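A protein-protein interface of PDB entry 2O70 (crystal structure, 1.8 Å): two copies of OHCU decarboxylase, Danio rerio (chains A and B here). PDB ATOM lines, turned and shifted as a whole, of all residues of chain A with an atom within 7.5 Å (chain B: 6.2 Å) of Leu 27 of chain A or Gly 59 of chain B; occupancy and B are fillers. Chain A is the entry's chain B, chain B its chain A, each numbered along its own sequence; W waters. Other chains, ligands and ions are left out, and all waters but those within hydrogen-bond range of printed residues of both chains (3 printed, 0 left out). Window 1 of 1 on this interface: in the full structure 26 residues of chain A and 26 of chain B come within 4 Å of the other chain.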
ATOM      1  N   VAL A  15     -15.772  -8.358  -9.993  1.00  0.00           N
ATOM      2  CA  VAL A  15     -16.159  -9.766 -10.086  1.00  0.00           C
ATOM      3  C   VAL A  15     -17.164 -10.168  -8.987  1.00  0.00           C
ATOM      4  O   VAL A  15     -18.111 -10.927  -9.234  1.00  0.00           O
ATOM      5  CB  VAL A  15     -14.908 -10.664 -10.057  1.00  0.00           C
ATOM      6  CG1 VAL A  15     -15.293 -12.151 -10.004  1.00  0.00           C
ATOM      7  CG2 VAL A  15     -14.048 -10.354 -11.280  1.00  0.00           C
ATOM      8  N   GLY A  19     -20.338 -11.029 -10.766  1.00  0.00           N
ATOM      9  CA  GLY A  19     -19.909 -12.388 -11.074  1.00  0.00           C
ATOM     10  C   GLY A  19     -21.022 -13.396 -11.314  1.00  0.00           C
ATOM     11  O   GLY A  19     -20.761 -14.494 -11.800  1.00  0.00           O
ATOM     12  N   VAL A  22     -24.303 -13.849 -15.343  1.00  0.00           N
ATOM     13  CA  VAL A  22     -24.501 -15.092 -16.070  1.00  0.00           C
ATOM     14  C   VAL A  22     -24.312 -16.230 -15.068  1.00  0.00           C
ATOM     15  O   VAL A  22     -23.237 -16.409 -14.493  1.00  0.00           O
ATOM     16  CB  VAL A  22     -23.557 -15.279 -17.270  1.00  0.00           C
ATOM     17  CG1 VAL A  22     -23.849 -16.614 -17.974  1.00  0.00           C
ATOM     18  CG2 VAL A  22     -23.725 -14.106 -18.280  1.00  0.00           C
ATOM     19  N   LYS A  24     -23.524 -18.832 -12.594  1.00  0.00           N
ATOM     20  CA  LYS A  24     -22.318 -19.593 -12.287  1.00  0.00           C
ATOM     21  C   LYS A  24     -21.193 -19.435 -13.299  1.00  0.00           C
ATOM     22  O   LYS A  24     -20.318 -20.309 -13.416  1.00  0.00           O
ATOM     23  CB  LYS A  24     -22.667 -21.070 -12.077  1.00  0.00           C
ATOM     24  CG  LYS A  24     -23.395 -21.315 -10.762  1.00  0.00           C
ATOM     25  CD  LYS A  24     -23.919 -22.740 -10.651  1.00  0.00           C
ATOM     26  CE  LYS A  24     -24.739 -22.913  -9.383  1.00  0.00           C
ATOM     27  NZ  LYS A  24     -25.146 -24.349  -9.190  1.00  0.00           N
ATOM     28  N   CYS A  25     -21.182 -18.303 -13.998  1.00  0.00           N
ATOM     29  CA  CYS A  25     -20.121 -18.033 -14.961  1.00  0.00           C
ATOM     30  C   CYS A  25     -19.400 -16.709 -14.688  1.00  0.00           C
ATOM     31  O   CYS A  25     -19.459 -15.811 -15.513  1.00  0.00           O
ATOM     32  CB  CYS A  25     -20.695 -18.011 -16.377  1.00  0.00           C
ATOM     33  SG  CYS A  25     -21.318 -19.623 -16.981  1.00  0.00           S
ATOM     34  N   PRO A  26     -18.717 -16.596 -13.531  1.00  0.00           N
ATOM     35  CA  PRO A  26     -18.000 -15.360 -13.200  1.00  0.00           C
ATOM     36  C   PRO A  26     -16.910 -15.037 -14.208  1.00  0.00           C
ATOM     37  O   PRO A  26     -16.502 -13.865 -14.318  1.00  0.00           O
ATOM     38  CB  PRO A  26     -17.392 -15.651 -11.828  1.00  0.00           C
ATOM     39  CG  PRO A  26     -17.363 -17.160 -11.713  1.00  0.00           C
ATOM     40  CD  PRO A  26     -18.592 -17.618 -12.476  1.00  0.00           C
ATOM     41  N   LEU A  27     -16.445 -16.054 -14.940  1.00  0.00           N
ATOM     42  CA  LEU A  27     -15.429 -15.845 -15.971  1.00  0.00           C
ATOM     43  C   LEU A  27     -15.845 -14.777 -16.967  1.00  0.00           C
ATOM     44  O   LEU A  27     -15.017 -13.984 -17.438  1.00  0.00           O
ATOM     45  CB  LEU A  27     -15.157 -17.138 -16.762  1.00  0.00           C
ATOM     46  CG  LEU A  27     -14.694 -16.725 -18.157  1.00  0.00           C
ATOM     47  CD1 LEU A  27     -13.225 -16.285 -18.081  1.00  0.00           C
ATOM     48  CD2 LEU A  27     -14.896 -17.769 -19.214  1.00  0.00           C
ATOM     49  N   ILE A  28     -17.124 -14.768 -17.311  1.00  0.00           N
ATOM     50  CA  ILE A  28     -17.609 -13.863 -18.357  1.00  0.00           C
ATOM     51  C   ILE A  28     -17.551 -12.404 -17.878  1.00  0.00           C
ATOM     52  O   ILE A  28     -17.008 -11.548 -18.564  1.00  0.00           O
ATOM     53  CB  ILE A  28     -19.022 -14.291 -18.831  1.00  0.00           C
ATOM     54  CG1 ILE A  28     -18.960 -15.708 -19.431  1.00  0.00           C
ATOM     55  CG2 ILE A  28     -19.598 -13.298 -19.829  1.00  0.00           C
ATOM     56  CD1 ILE A  28     -20.281 -16.231 -19.903  1.00  0.00           C
ATOM     57  N   SER A  29     -18.069 -12.142 -16.686  1.00  0.00           N
ATOM     58  CA  SER A  29     -17.987 -10.808 -16.112  1.00  0.00           C
ATOM     59  C   SER A  29     -16.544 -10.419 -15.804  1.00  0.00           C
ATOM     60  O   SER A  29     -16.153  -9.270 -16.019  1.00  0.00           O
ATOM     61  CB  SER A  29     -18.874 -10.693 -14.868  1.00  0.00           C
ATOM     62  OG  SER A  29     -18.300 -11.342 -13.749  1.00  0.00           O
ATOM     63  N   ALA A  30     -15.744 -11.376 -15.331  1.00  0.00           N
ATOM     64  CA  ALA A  30     -14.322 -11.103 -15.077  1.00  0.00           C
ATOM     65  C   ALA A  30     -13.610 -10.704 -16.372  1.00  0.00           C
ATOM     66  O   ALA A  30     -12.737  -9.834 -16.358  1.00  0.00           O
ATOM     67  CB  ALA A  30     -13.634 -12.314 -14.440  1.00  0.00           C
ATOM     68  N   ALA A  31     -13.959 -11.366 -17.479  1.00  0.00           N
ATOM     69  CA  ALA A  31     -13.343 -11.090 -18.776  1.00  0.00           C
ATOM     70  C   ALA A  31     -13.619  -9.662 -19.232  1.00  0.00           C
ATOM     71  O   ALA A  31     -12.716  -8.929 -19.645  1.00  0.00           O
ATOM     72  CB  ALA A  31     -13.847 -12.072 -19.823  1.00  0.00           C
ATOM     73  N   ILE A  32     -14.868  -9.246 -19.163  1.00  0.00           N
ATOM     74  CA  ILE A  32     -15.191  -7.964 -19.764  1.00  0.00           C
ATOM     75  C   ILE A  32     -14.635  -6.747 -18.990  1.00  0.00           C
ATOM     76  O   ILE A  32     -14.617  -5.634 -19.534  1.00  0.00           O
ATOM     77  CB  ILE A  32     -16.711  -7.848 -20.072  1.00  0.00           C
ATOM     78  CG1 ILE A  32     -17.533  -8.071 -18.805  1.00  0.00           C
ATOM     79  CG2 ILE A  32     -17.120  -8.861 -21.151  1.00  0.00           C
ATOM     80  CD1 ILE A  32     -17.876  -6.796 -18.098  1.00  0.00           C
ATOM     81  N   TRP A  33     -14.187  -6.949 -17.748  1.00  0.00           N
ATOM     82  CA  TRP A  33     -13.520  -5.875 -16.976  1.00  0.00           C
ATOM     83  C   TRP A  33     -12.298  -5.339 -17.742  1.00  0.00           C
ATOM     84  O   TRP A  33     -11.879  -4.199 -17.533  1.00  0.00           O
ATOM     85  CB  TRP A  33     -13.130  -6.369 -15.567  1.00  0.00           C
ATOM     86  CG  TRP A  33     -12.480  -5.342 -14.642  1.00  0.00           C
ATOM     87  CD1 TRP A  33     -13.114  -4.448 -13.830  1.00  0.00           C
ATOM     88  CD2 TRP A  33     -11.071  -5.163 -14.411  1.00  0.00           C
ATOM     89  NE1 TRP A  33     -12.187  -3.703 -13.118  1.00  0.00           N
ATOM     90  CE2 TRP A  33     -10.928  -4.119 -13.464  1.00  0.00           C
ATOM     91  CE3 TRP A  33      -9.914  -5.773 -14.926  1.00  0.00           C
ATOM     92  CZ2 TRP A  33      -9.684  -3.686 -13.019  1.00  0.00           C
ATOM     93  CZ3 TRP A  33      -8.668  -5.327 -14.480  1.00  0.00           C
ATOM     94  CH2 TRP A  33      -8.569  -4.299 -13.541  1.00  0.00           C
ATOM     95  N   SER A  34     -11.733  -6.168 -18.620  1.00  0.00           N
ATOM     96  CA  SER A  34     -10.633  -5.768 -19.493  1.00  0.00           C
ATOM     97  C   SER A  34     -10.996  -4.628 -20.454  1.00  0.00           C
ATOM     98  O   SER A  34     -10.097  -3.980 -21.028  1.00  0.00           O
ATOM     99  CB  SER A  34     -10.160  -6.965 -20.336  1.00  0.00           C
ATOM    100  OG  SER A  34      -9.360  -7.853 -19.586  1.00  0.00           O
ATOM    101  N   TYR A  35     -12.292  -4.375 -20.636  1.00  0.00           N
ATOM    102  CA  TYR A  35     -12.731  -3.383 -21.609  1.00  0.00           C
ATOM    103  C   TYR A  35     -13.151  -2.044 -20.986  1.00  0.00           C
ATOM    104  O   TYR A  35     -13.675  -1.166 -21.680  1.00  0.00           O
ATOM    105  CB  TYR A  35     -13.868  -3.946 -22.457  1.00  0.00           C
ATOM    106  CG  TYR A  35     -13.517  -5.219 -23.181  1.00  0.00           C
ATOM    107  CD1 TYR A  35     -12.475  -5.248 -24.095  1.00  0.00           C
ATOM    108  CD2 TYR A  35     -14.235  -6.387 -22.960  1.00  0.00           C
ATOM    109  CE1 TYR A  35     -12.145  -6.413 -24.767  1.00  0.00           C
ATOM    110  CE2 TYR A  35     -13.914  -7.563 -23.630  1.00  0.00           C
ATOM    111  CZ  TYR A  35     -12.862  -7.568 -24.524  1.00  0.00           C
ATOM    112  OH  TYR A  35     -12.535  -8.722 -25.206  1.00  0.00           O
ATOM    113  N   PHE A  51     -18.941 -11.234 -25.993  1.00  0.00           N
ATOM    114  CA  PHE A  51     -18.143 -12.324 -25.446  1.00  0.00           C
ATOM    115  C   PHE A  51     -18.835 -13.679 -25.656  1.00  0.00           C
ATOM    116  O   PHE A  51     -18.235 -14.614 -26.174  1.00  0.00           O
ATOM    117  CB  PHE A  51     -17.856 -12.119 -23.951  1.00  0.00           C
ATOM    118  CG  PHE A  51     -16.900 -13.122 -23.397  1.00  0.00           C
ATOM    119  CD1 PHE A  51     -15.521 -12.851 -23.366  1.00  0.00           C
ATOM    120  CD2 PHE A  51     -17.355 -14.336 -22.908  1.00  0.00           C
ATOM    121  CE1 PHE A  51     -14.630 -13.790 -22.877  1.00  0.00           C
ATOM    122  CE2 PHE A  51     -16.462 -15.287 -22.412  1.00  0.00           C
ATOM    123  CZ  PHE A  51     -15.103 -15.004 -22.380  1.00  0.00           C
ATOM    124  N   LEU A  55     -17.770 -17.376 -28.302  1.00  0.00           N
ATOM    125  CA  LEU A  55     -17.527 -18.744 -27.834  1.00  0.00           C
ATOM    126  C   LEU A  55     -17.852 -19.790 -28.886  1.00  0.00           C
ATOM    127  O   LEU A  55     -18.763 -19.591 -29.700  1.00  0.00           O
ATOM    128  CB  LEU A  55     -18.345 -19.036 -26.577  1.00  0.00           C
ATOM    129  CG  LEU A  55     -18.050 -18.198 -25.332  1.00  0.00           C
ATOM    130  CD1 LEU A  55     -19.071 -18.513 -24.225  1.00  0.00           C
ATOM    131  CD2 LEU A  55     -16.619 -18.412 -24.831  1.00  0.00           C
ATOM    132  N   LYS B  24     -13.322 -22.111 -10.131  1.00  0.00           N
ATOM    133  CA  LYS B  24     -14.572 -21.346 -10.298  1.00  0.00           C
ATOM    134  C   LYS B  24     -14.972 -21.156 -11.763  1.00  0.00           C
ATOM    135  O   LYS B  24     -15.653 -20.190 -12.115  1.00  0.00           O
ATOM    136  CB  LYS B  24     -14.509 -20.002  -9.552  1.00  0.00           C
ATOM    137  CG  LYS B  24     -14.273 -20.171  -8.045  1.00  0.00           C
ATOM    138  CD  LYS B  24     -14.460 -18.869  -7.285  1.00  0.00           C
ATOM    139  CE  LYS B  24     -14.127 -19.087  -5.808  1.00  0.00           C
ATOM    140  NZ  LYS B  24     -13.959 -17.769  -5.111  1.00  0.00           N
ATOM    141  N   CYS B  25     -14.542 -22.092 -12.612  1.00  0.00           N
ATOM    142  CA  CYS B  25     -14.906 -22.073 -14.021  1.00  0.00           C
ATOM    143  C   CYS B  25     -15.591 -23.379 -14.450  1.00  0.00           C
ATOM    144  O   CYS B  25     -15.064 -24.121 -15.304  1.00  0.00           O
ATOM    145  CB  CYS B  25     -13.678 -21.807 -14.891  1.00  0.00           C
ATOM    146  SG  CYS B  25     -12.982 -20.150 -14.653  1.00  0.00           S
ATOM    147  N   LEU B  27     -17.938 -23.686 -16.349  1.00  0.00           N
ATOM    148  CA  LEU B  27     -18.264 -23.540 -17.760  1.00  0.00           C
ATOM    149  C   LEU B  27     -17.322 -24.355 -18.643  1.00  0.00           C
ATOM    150  O   LEU B  27     -17.716 -24.915 -19.676  1.00  0.00           O
ATOM    151  CB  LEU B  27     -18.157 -22.057 -18.143  1.00  0.00           C
ATOM    152  CG  LEU B  27     -18.168 -21.744 -19.621  1.00  0.00           C
ATOM    153  CD1 LEU B  27     -19.400 -22.425 -20.221  1.00  0.00           C
ATOM    154  CD2 LEU B  27     -18.222 -20.241 -19.816  1.00  0.00           C
ATOM    155  N   ILE B  28     -16.063 -24.419 -18.231  1.00  0.00           N
ATOM    156  CA  ILE B  28     -15.061 -25.133 -19.018  1.00  0.00           C
ATOM    157  C   ILE B  28     -15.326 -26.639 -19.043  1.00  0.00           C
ATOM    158  O   ILE B  28     -15.318 -27.256 -20.112  1.00  0.00           O
ATOM    159  CB  ILE B  28     -13.650 -24.819 -18.511  1.00  0.00           C
ATOM    160  CG1 ILE B  28     -13.323 -23.347 -18.779  1.00  0.00           C
ATOM    161  CG2 ILE B  28     -12.606 -25.764 -19.161  1.00  0.00           C
ATOM    162  CD1 ILE B  28     -12.122 -22.866 -18.010  1.00  0.00           C
ATOM    163  N   PHE B  51     -10.055 -25.419 -25.605  1.00  0.00           N
ATOM    164  CA  PHE B  51     -11.124 -24.498 -25.261  1.00  0.00           C
ATOM    165  C   PHE B  51     -10.561 -23.173 -24.759  1.00  0.00           C
ATOM    166  O   PHE B  51     -10.971 -22.103 -25.205  1.00  0.00           O
ATOM    167  CB  PHE B  51     -12.039 -25.091 -24.189  1.00  0.00           C
ATOM    168  CG  PHE B  51     -13.248 -24.239 -23.917  1.00  0.00           C
ATOM    169  CD1 PHE B  51     -14.398 -24.376 -24.682  1.00  0.00           C
ATOM    170  CD2 PHE B  51     -13.220 -23.285 -22.912  1.00  0.00           C
ATOM    171  CE1 PHE B  51     -15.497 -23.577 -24.449  1.00  0.00           C
ATOM    172  CE2 PHE B  51     -14.320 -22.482 -22.660  1.00  0.00           C
ATOM    173  CZ  PHE B  51     -15.463 -22.629 -23.432  1.00  0.00           C
ATOM    174  N   LEU B  55     -10.391 -18.913 -26.511  1.00  0.00           N
ATOM    175  CA  LEU B  55     -10.997 -17.716 -25.935  1.00  0.00           C
ATOM    176  C   LEU B  55     -10.226 -16.480 -26.349  1.00  0.00           C
ATOM    177  O   LEU B  55      -9.041 -16.574 -26.647  1.00  0.00           O
ATOM    178  CB  LEU B  55     -11.000 -17.792 -24.403  1.00  0.00           C
ATOM    179  CG  LEU B  55     -11.686 -18.982 -23.737  1.00  0.00           C
ATOM    180  CD1 LEU B  55     -11.433 -18.928 -22.236  1.00  0.00           C
ATOM    181  CD2 LEU B  55     -13.176 -18.962 -24.026  1.00  0.00           C
ATOM    182  N   PRO B  56     -10.892 -15.307 -26.359  1.00  0.00           N
ATOM    183  CA  PRO B  56     -10.137 -14.077 -26.542  1.00  0.00           C
ATOM    184  C   PRO B  56      -9.223 -13.883 -25.340  1.00  0.00           C
ATOM    185  O   PRO B  56      -9.425 -14.537 -24.301  1.00  0.00           O
ATOM    186  CB  PRO B  56     -11.223 -12.988 -26.597  1.00  0.00           C
ATOM    187  CG  PRO B  56     -12.409 -13.575 -25.964  1.00  0.00           C
ATOM    188  CD  PRO B  56     -12.337 -15.058 -26.217  1.00  0.00           C
ATOM    189  N   ASP B  57      -8.208 -13.039 -25.491  1.00  0.00           N
ATOM    190  CA  ASP B  57      -7.309 -12.720 -24.384  1.00  0.00           C
ATOM    191  C   ASP B  57      -8.074 -12.312 -23.116  1.00  0.00           C
ATOM    192  O   ASP B  57      -7.663 -12.644 -22.008  1.00  0.00           O
ATOM    193  CB  ASP B  57      -6.345 -11.603 -24.777  1.00  0.00           C
ATOM    194  CG  ASP B  57      -5.128 -12.115 -25.555  1.00  0.00           C
ATOM    195  OD1 ASP B  57      -4.844 -13.339 -25.551  1.00  0.00           O
ATOM    196  OD2 ASP B  57      -4.442 -11.272 -26.160  1.00  0.00           O
ATOM    197  N   SER B  58      -9.177 -11.583 -23.290  1.00  0.00           N
ATOM    198  CA  SER B  58      -9.988 -11.153 -22.147  1.00  0.00           C
ATOM    199  C   SER B  58     -10.561 -12.366 -21.397  1.00  0.00           C
ATOM    200  O   SER B  58     -10.712 -12.331 -20.188  1.00  0.00           O
ATOM    201  CB  SER B  58     -11.109 -10.212 -22.595  1.00  0.00           C
ATOM    202  OG  SER B  58     -12.064 -10.887 -23.421  1.00  0.00           O
ATOM    203  N   GLY B  59     -10.876 -13.434 -22.131  1.00  0.00           N
ATOM    204  CA  GLY B  59     -11.379 -14.675 -21.520  1.00  0.00           C
ATOM    205  C   GLY B  59     -10.313 -15.349 -20.701  1.00  0.00           C
ATOM    206  O   GLY B  59     -10.576 -15.856 -19.616  1.00  0.00           O
ATOM    207  N   LYS B  60      -9.090 -15.335 -21.228  1.00  0.00           N
ATOM    208  CA  LYS B  60      -7.945 -15.865 -20.510  1.00  0.00           C
ATOM    209  C   LYS B  60      -7.704 -15.076 -19.205  1.00  0.00           C
ATOM    210  O   LYS B  60      -7.554 -15.677 -18.144  1.00  0.00           O
ATOM    211  CB  LYS B  60      -6.720 -15.892 -21.429  1.00  0.00           C
ATOM    212  CG  LYS B  60      -6.836 -16.936 -22.554  1.00  0.00           C
ATOM    213  CD  LYS B  60      -5.600 -16.911 -23.461  1.00  0.00           C
ATOM    214  CE  LYS B  60      -5.759 -17.872 -24.639  1.00  0.00           C
ATOM    215  NZ  LYS B  60      -5.634 -19.279 -24.135  1.00  0.00           N
ATOM    216  N   GLU B  61      -7.745 -13.751 -19.283  1.00  0.00           N
ATOM    217  CA  GLU B  61      -7.626 -12.894 -18.091  1.00  0.00           C
ATOM    218  C   GLU B  61      -8.762 -13.156 -17.119  1.00  0.00           C
ATOM    219  O   GLU B  61      -8.553 -13.197 -15.913  1.00  0.00           O
ATOM    220  CB  GLU B  61      -7.614 -11.410 -18.477  1.00  0.00           C
ATOM    221  CG  GLU B  61      -6.445 -11.067 -19.360  1.00  0.00           C
ATOM    222  CD  GLU B  61      -6.549  -9.675 -19.924  1.00  0.00           C
ATOM    223  OE1 GLU B  61      -7.673  -9.252 -20.289  1.00  0.00           O
ATOM    224  OE2 GLU B  61      -5.499  -9.013 -19.992  1.00  0.00           O
ATOM    225  N   GLY B  62      -9.968 -13.330 -17.660  1.00  0.00           N
ATOM    226  CA  GLY B  62     -11.126 -13.675 -16.862  1.00  0.00           C
ATOM    227  C   GLY B  62     -10.930 -14.929 -16.015  1.00  0.00           C
ATOM    228  O   GLY B  62     -11.296 -14.960 -14.838  1.00  0.00           O
ATOM    229  N   ILE B  63     -10.392 -15.981 -16.635  1.00  0.00           N
ATOM    230  CA  ILE B  63     -10.109 -17.214 -15.938  1.00  0.00           C
ATOM    231  C   ILE B  63      -9.198 -16.916 -14.749  1.00  0.00           C
ATOM    232  O   ILE B  63      -9.449 -17.356 -13.630  1.00  0.00           O
ATOM    233  CB  ILE B  63      -9.487 -18.264 -16.875  1.00  0.00           C
ATOM    234  CG1 ILE B  63     -10.565 -18.777 -17.870  1.00  0.00           C
ATOM    235  CG2 ILE B  63      -8.890 -19.412 -16.062  1.00  0.00           C
ATOM    236  CD1 ILE B  63     -10.069 -19.796 -18.906  1.00  0.00           C
ATOM    237  N   LEU B  64      -8.164 -16.129 -14.998  1.00  0.00           N
ATOM    238  CA  LEU B  64      -7.181 -15.830 -13.967  1.00  0.00           C
ATOM    239  C   LEU B  64      -7.848 -15.070 -12.807  1.00  0.00           C
ATOM    240  O   LEU B  64      -7.594 -15.352 -11.629  1.00  0.00           O
ATOM    241  CB  LEU B  64      -6.035 -15.022 -14.566  1.00  0.00           C
ATOM    242  CG  LEU B  64      -5.153 -15.763 -15.591  1.00  0.00           C
ATOM    243  CD1 LEU B  64      -4.093 -14.838 -16.186  1.00  0.00           C
ATOM    244  CD2 LEU B  64      -4.523 -17.030 -14.954  1.00  0.00           C
ATOM    245  N   CYS B  66     -10.679 -15.349 -11.720  1.00  0.00           N
ATOM    246  CA  CYS B  66     -11.529 -16.234 -10.943  1.00  0.00           C
ATOM    247  C   CYS B  66     -10.742 -16.921  -9.825  1.00  0.00           C
ATOM    248  O   CYS B  66     -11.328 -17.590  -8.979  1.00  0.00           O
ATOM    249  CB  CYS B  66     -12.194 -17.270 -11.859  1.00  0.00           C
ATOM    250  SG  CYS B  66     -13.559 -16.565 -12.825  1.00  0.00           S
ATOM    251  N   ILE B 151      -1.508 -18.684 -17.802  1.00  0.00           N
ATOM    252  CA  ILE B 151      -2.424 -19.680 -18.375  1.00  0.00           C
ATOM    253  C   ILE B 151      -1.780 -21.074 -18.398  1.00  0.00           C
ATOM    254  O   ILE B 151      -2.420 -22.089 -18.124  1.00  0.00           O
ATOM    255  CB  ILE B 151      -2.930 -19.240 -19.763  1.00  0.00           C
ATOM    256  CG1 ILE B 151      -3.955 -18.107 -19.594  1.00  0.00           C
ATOM    257  CG2 ILE B 151      -3.584 -20.439 -20.524  1.00  0.00           C
ATOM    258  CD1 ILE B 151      -5.239 -18.580 -18.870  1.00  0.00           C
HETATM  259  O   HOH W   1     -18.263 -20.950 -15.313  1.00  0.00           O
HETATM  260  O   HOH W   2      -9.538  -9.894 -25.597  1.00  0.00           O
HETATM  261  O   HOH W   3     -16.460 -18.945 -14.513  1.00  0.00           O
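Among the printed residues, pairs that only touch across the chains: Pro 26 of chain A with Lys 24 of chain B (3.5 Å), Pro 26 of chain A with Cys 66 of chain B (3.9 Å), Leu 27 of chain A with Gly 59 of chain B (3.1 Å), Leu 27 of chain A with Gly 62 of chain B (3.4 Å), Leu 27 of chain A with Ile 63 of chain B (3.2 Å), Ala 30 of chain A with Gly 62 of chain B (3.6 Å), Ala 31 of chain A with Ser 58 of chain B (3.2 Å), Ala 31 of chain A with Gly 59 of chain B (3.97 Å), Ala 31 of chain A with Gly 62 of chain B (3.7 Å), Phe 51 of chain A with Pro 56 of chain B (3.8 Å), Phe 51 of chain A with Ser 58 of chain B (3.9 Å), Phe 51 of chain A with Gly 59 of chain B (3.6 Å) and Leu 55 of chain A with Leu 55 of chain B (3.6 Å).
Hydrophobic or aromatic side chains of chain A that line the printed part of chain B: Pro 26, Leu 27, Ala 30, Ala 31, Tyr 35, Phe 51 and Leu 55. Of the 17 printed residues of chain B, 9 touch a printed residue of chain A. Among the printed residues, 16 pairs touch across the chains. Among the printed residues, no Asp or Glu carboxylate lies within 4 Å of a Lys or Arg side-chain nitrogen of the other chain.
Of chain B, only Gly 59 (3.1 Å), Gly 62 (3.4 Å), Ile 63 (3.2 Å) and Cys 66 (3.6 Å) come within 4 Å of Leu 27 of chain A. Gly 59 of chain B touches just these residues of chain A: Leu 27 (3.1 Å), Ala 31 (3.97 Å) and Phe 51 (3.6 Å). Of chain A, only Ala 31 (3.2 Å), Tyr 35 (2.8 Å) and Phe 51 (3.9 Å) come within 4 Å of Ser 58 of chain B. Of the printed residues of chain A, Pro 56 of chain B touches Phe 51. Printed residues of chain A within 4 Å of Glu 61 of chain B: Ser 34 (2.3 Å). Of the printed residues of chain A, Gly 62 of chain B touches Leu 27, Ala 30 and Ala 31. Printed residues of chain A within 4 Å of Ile 63 of chain B: Leu 27 (3.2 Å). Printed residues of chain B within 4 Å of Leu 55 of chain A: Leu 55. Cys 25 of chain B touches none of the printed residues of chain A. Asp 57 of chain B touches none of the printed residues of chain A. The nearest residue of chain B that does not touch Leu 27 of chain A is Leu 27 of chain B (4.2 Å).
Water W3 lies within hydrogen-bond range of the backbone carbonyl oxygen (O) of Lys 24 of chain B (2.8 Å), the backbone NH (N) of Leu 27 of chain A (2.9 Å) and the side-chain sulfur (SG) of Cys 25 of chain B (3.7 Å). Water W1 lies within hydrogen-bond range of the backbone carbonyl oxygen (O) of Lys 24 of chain A (2.9 Å), the backbone NH (N) of Leu 27 of chain B (2.9 Å) and the side-chain sulfur (SG) of Cys 25 of chain A (3.7 Å). Water W2 lies within hydrogen-bond range of N of Ser 58 of chain B, OH of Tyr 35 of chain A and N of Asp 57 of chain B.
Leu 55 of chain B touches its own counterpart, Leu 55 of chain A. Of the 16 pairs that touch across the chains among the printed residues, 1 has its exchanged pair printed and touching as well.
The backbone carbonyl oxygen of Gly 62 of chain B sits at hydrogen-bond distance from the side-chain sulfur of Cys 66 of chain B (3.4 Å). The backbone carbonyl oxygen of Pro 26 of chain A sits at hydrogen-bond distance from the side-chain hydroxyl of Ser 29 of chain A, at 3.1 Å.
The side-chain hydroxyl (OH) of Tyr 35 of chain A sits at hydrogen-bond distance from the side-chain hydroxyl (OG) of Ser 58 of chain B, at 2.8 Å. SG of Cys 66 of chain B sits at hydrogen-bond distance from N of Leu 27 of chain A, 3.6 Å away. OG of Ser 34 of chain A lies close to OE1 of Glu 61 of chain B (2.3 Å).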
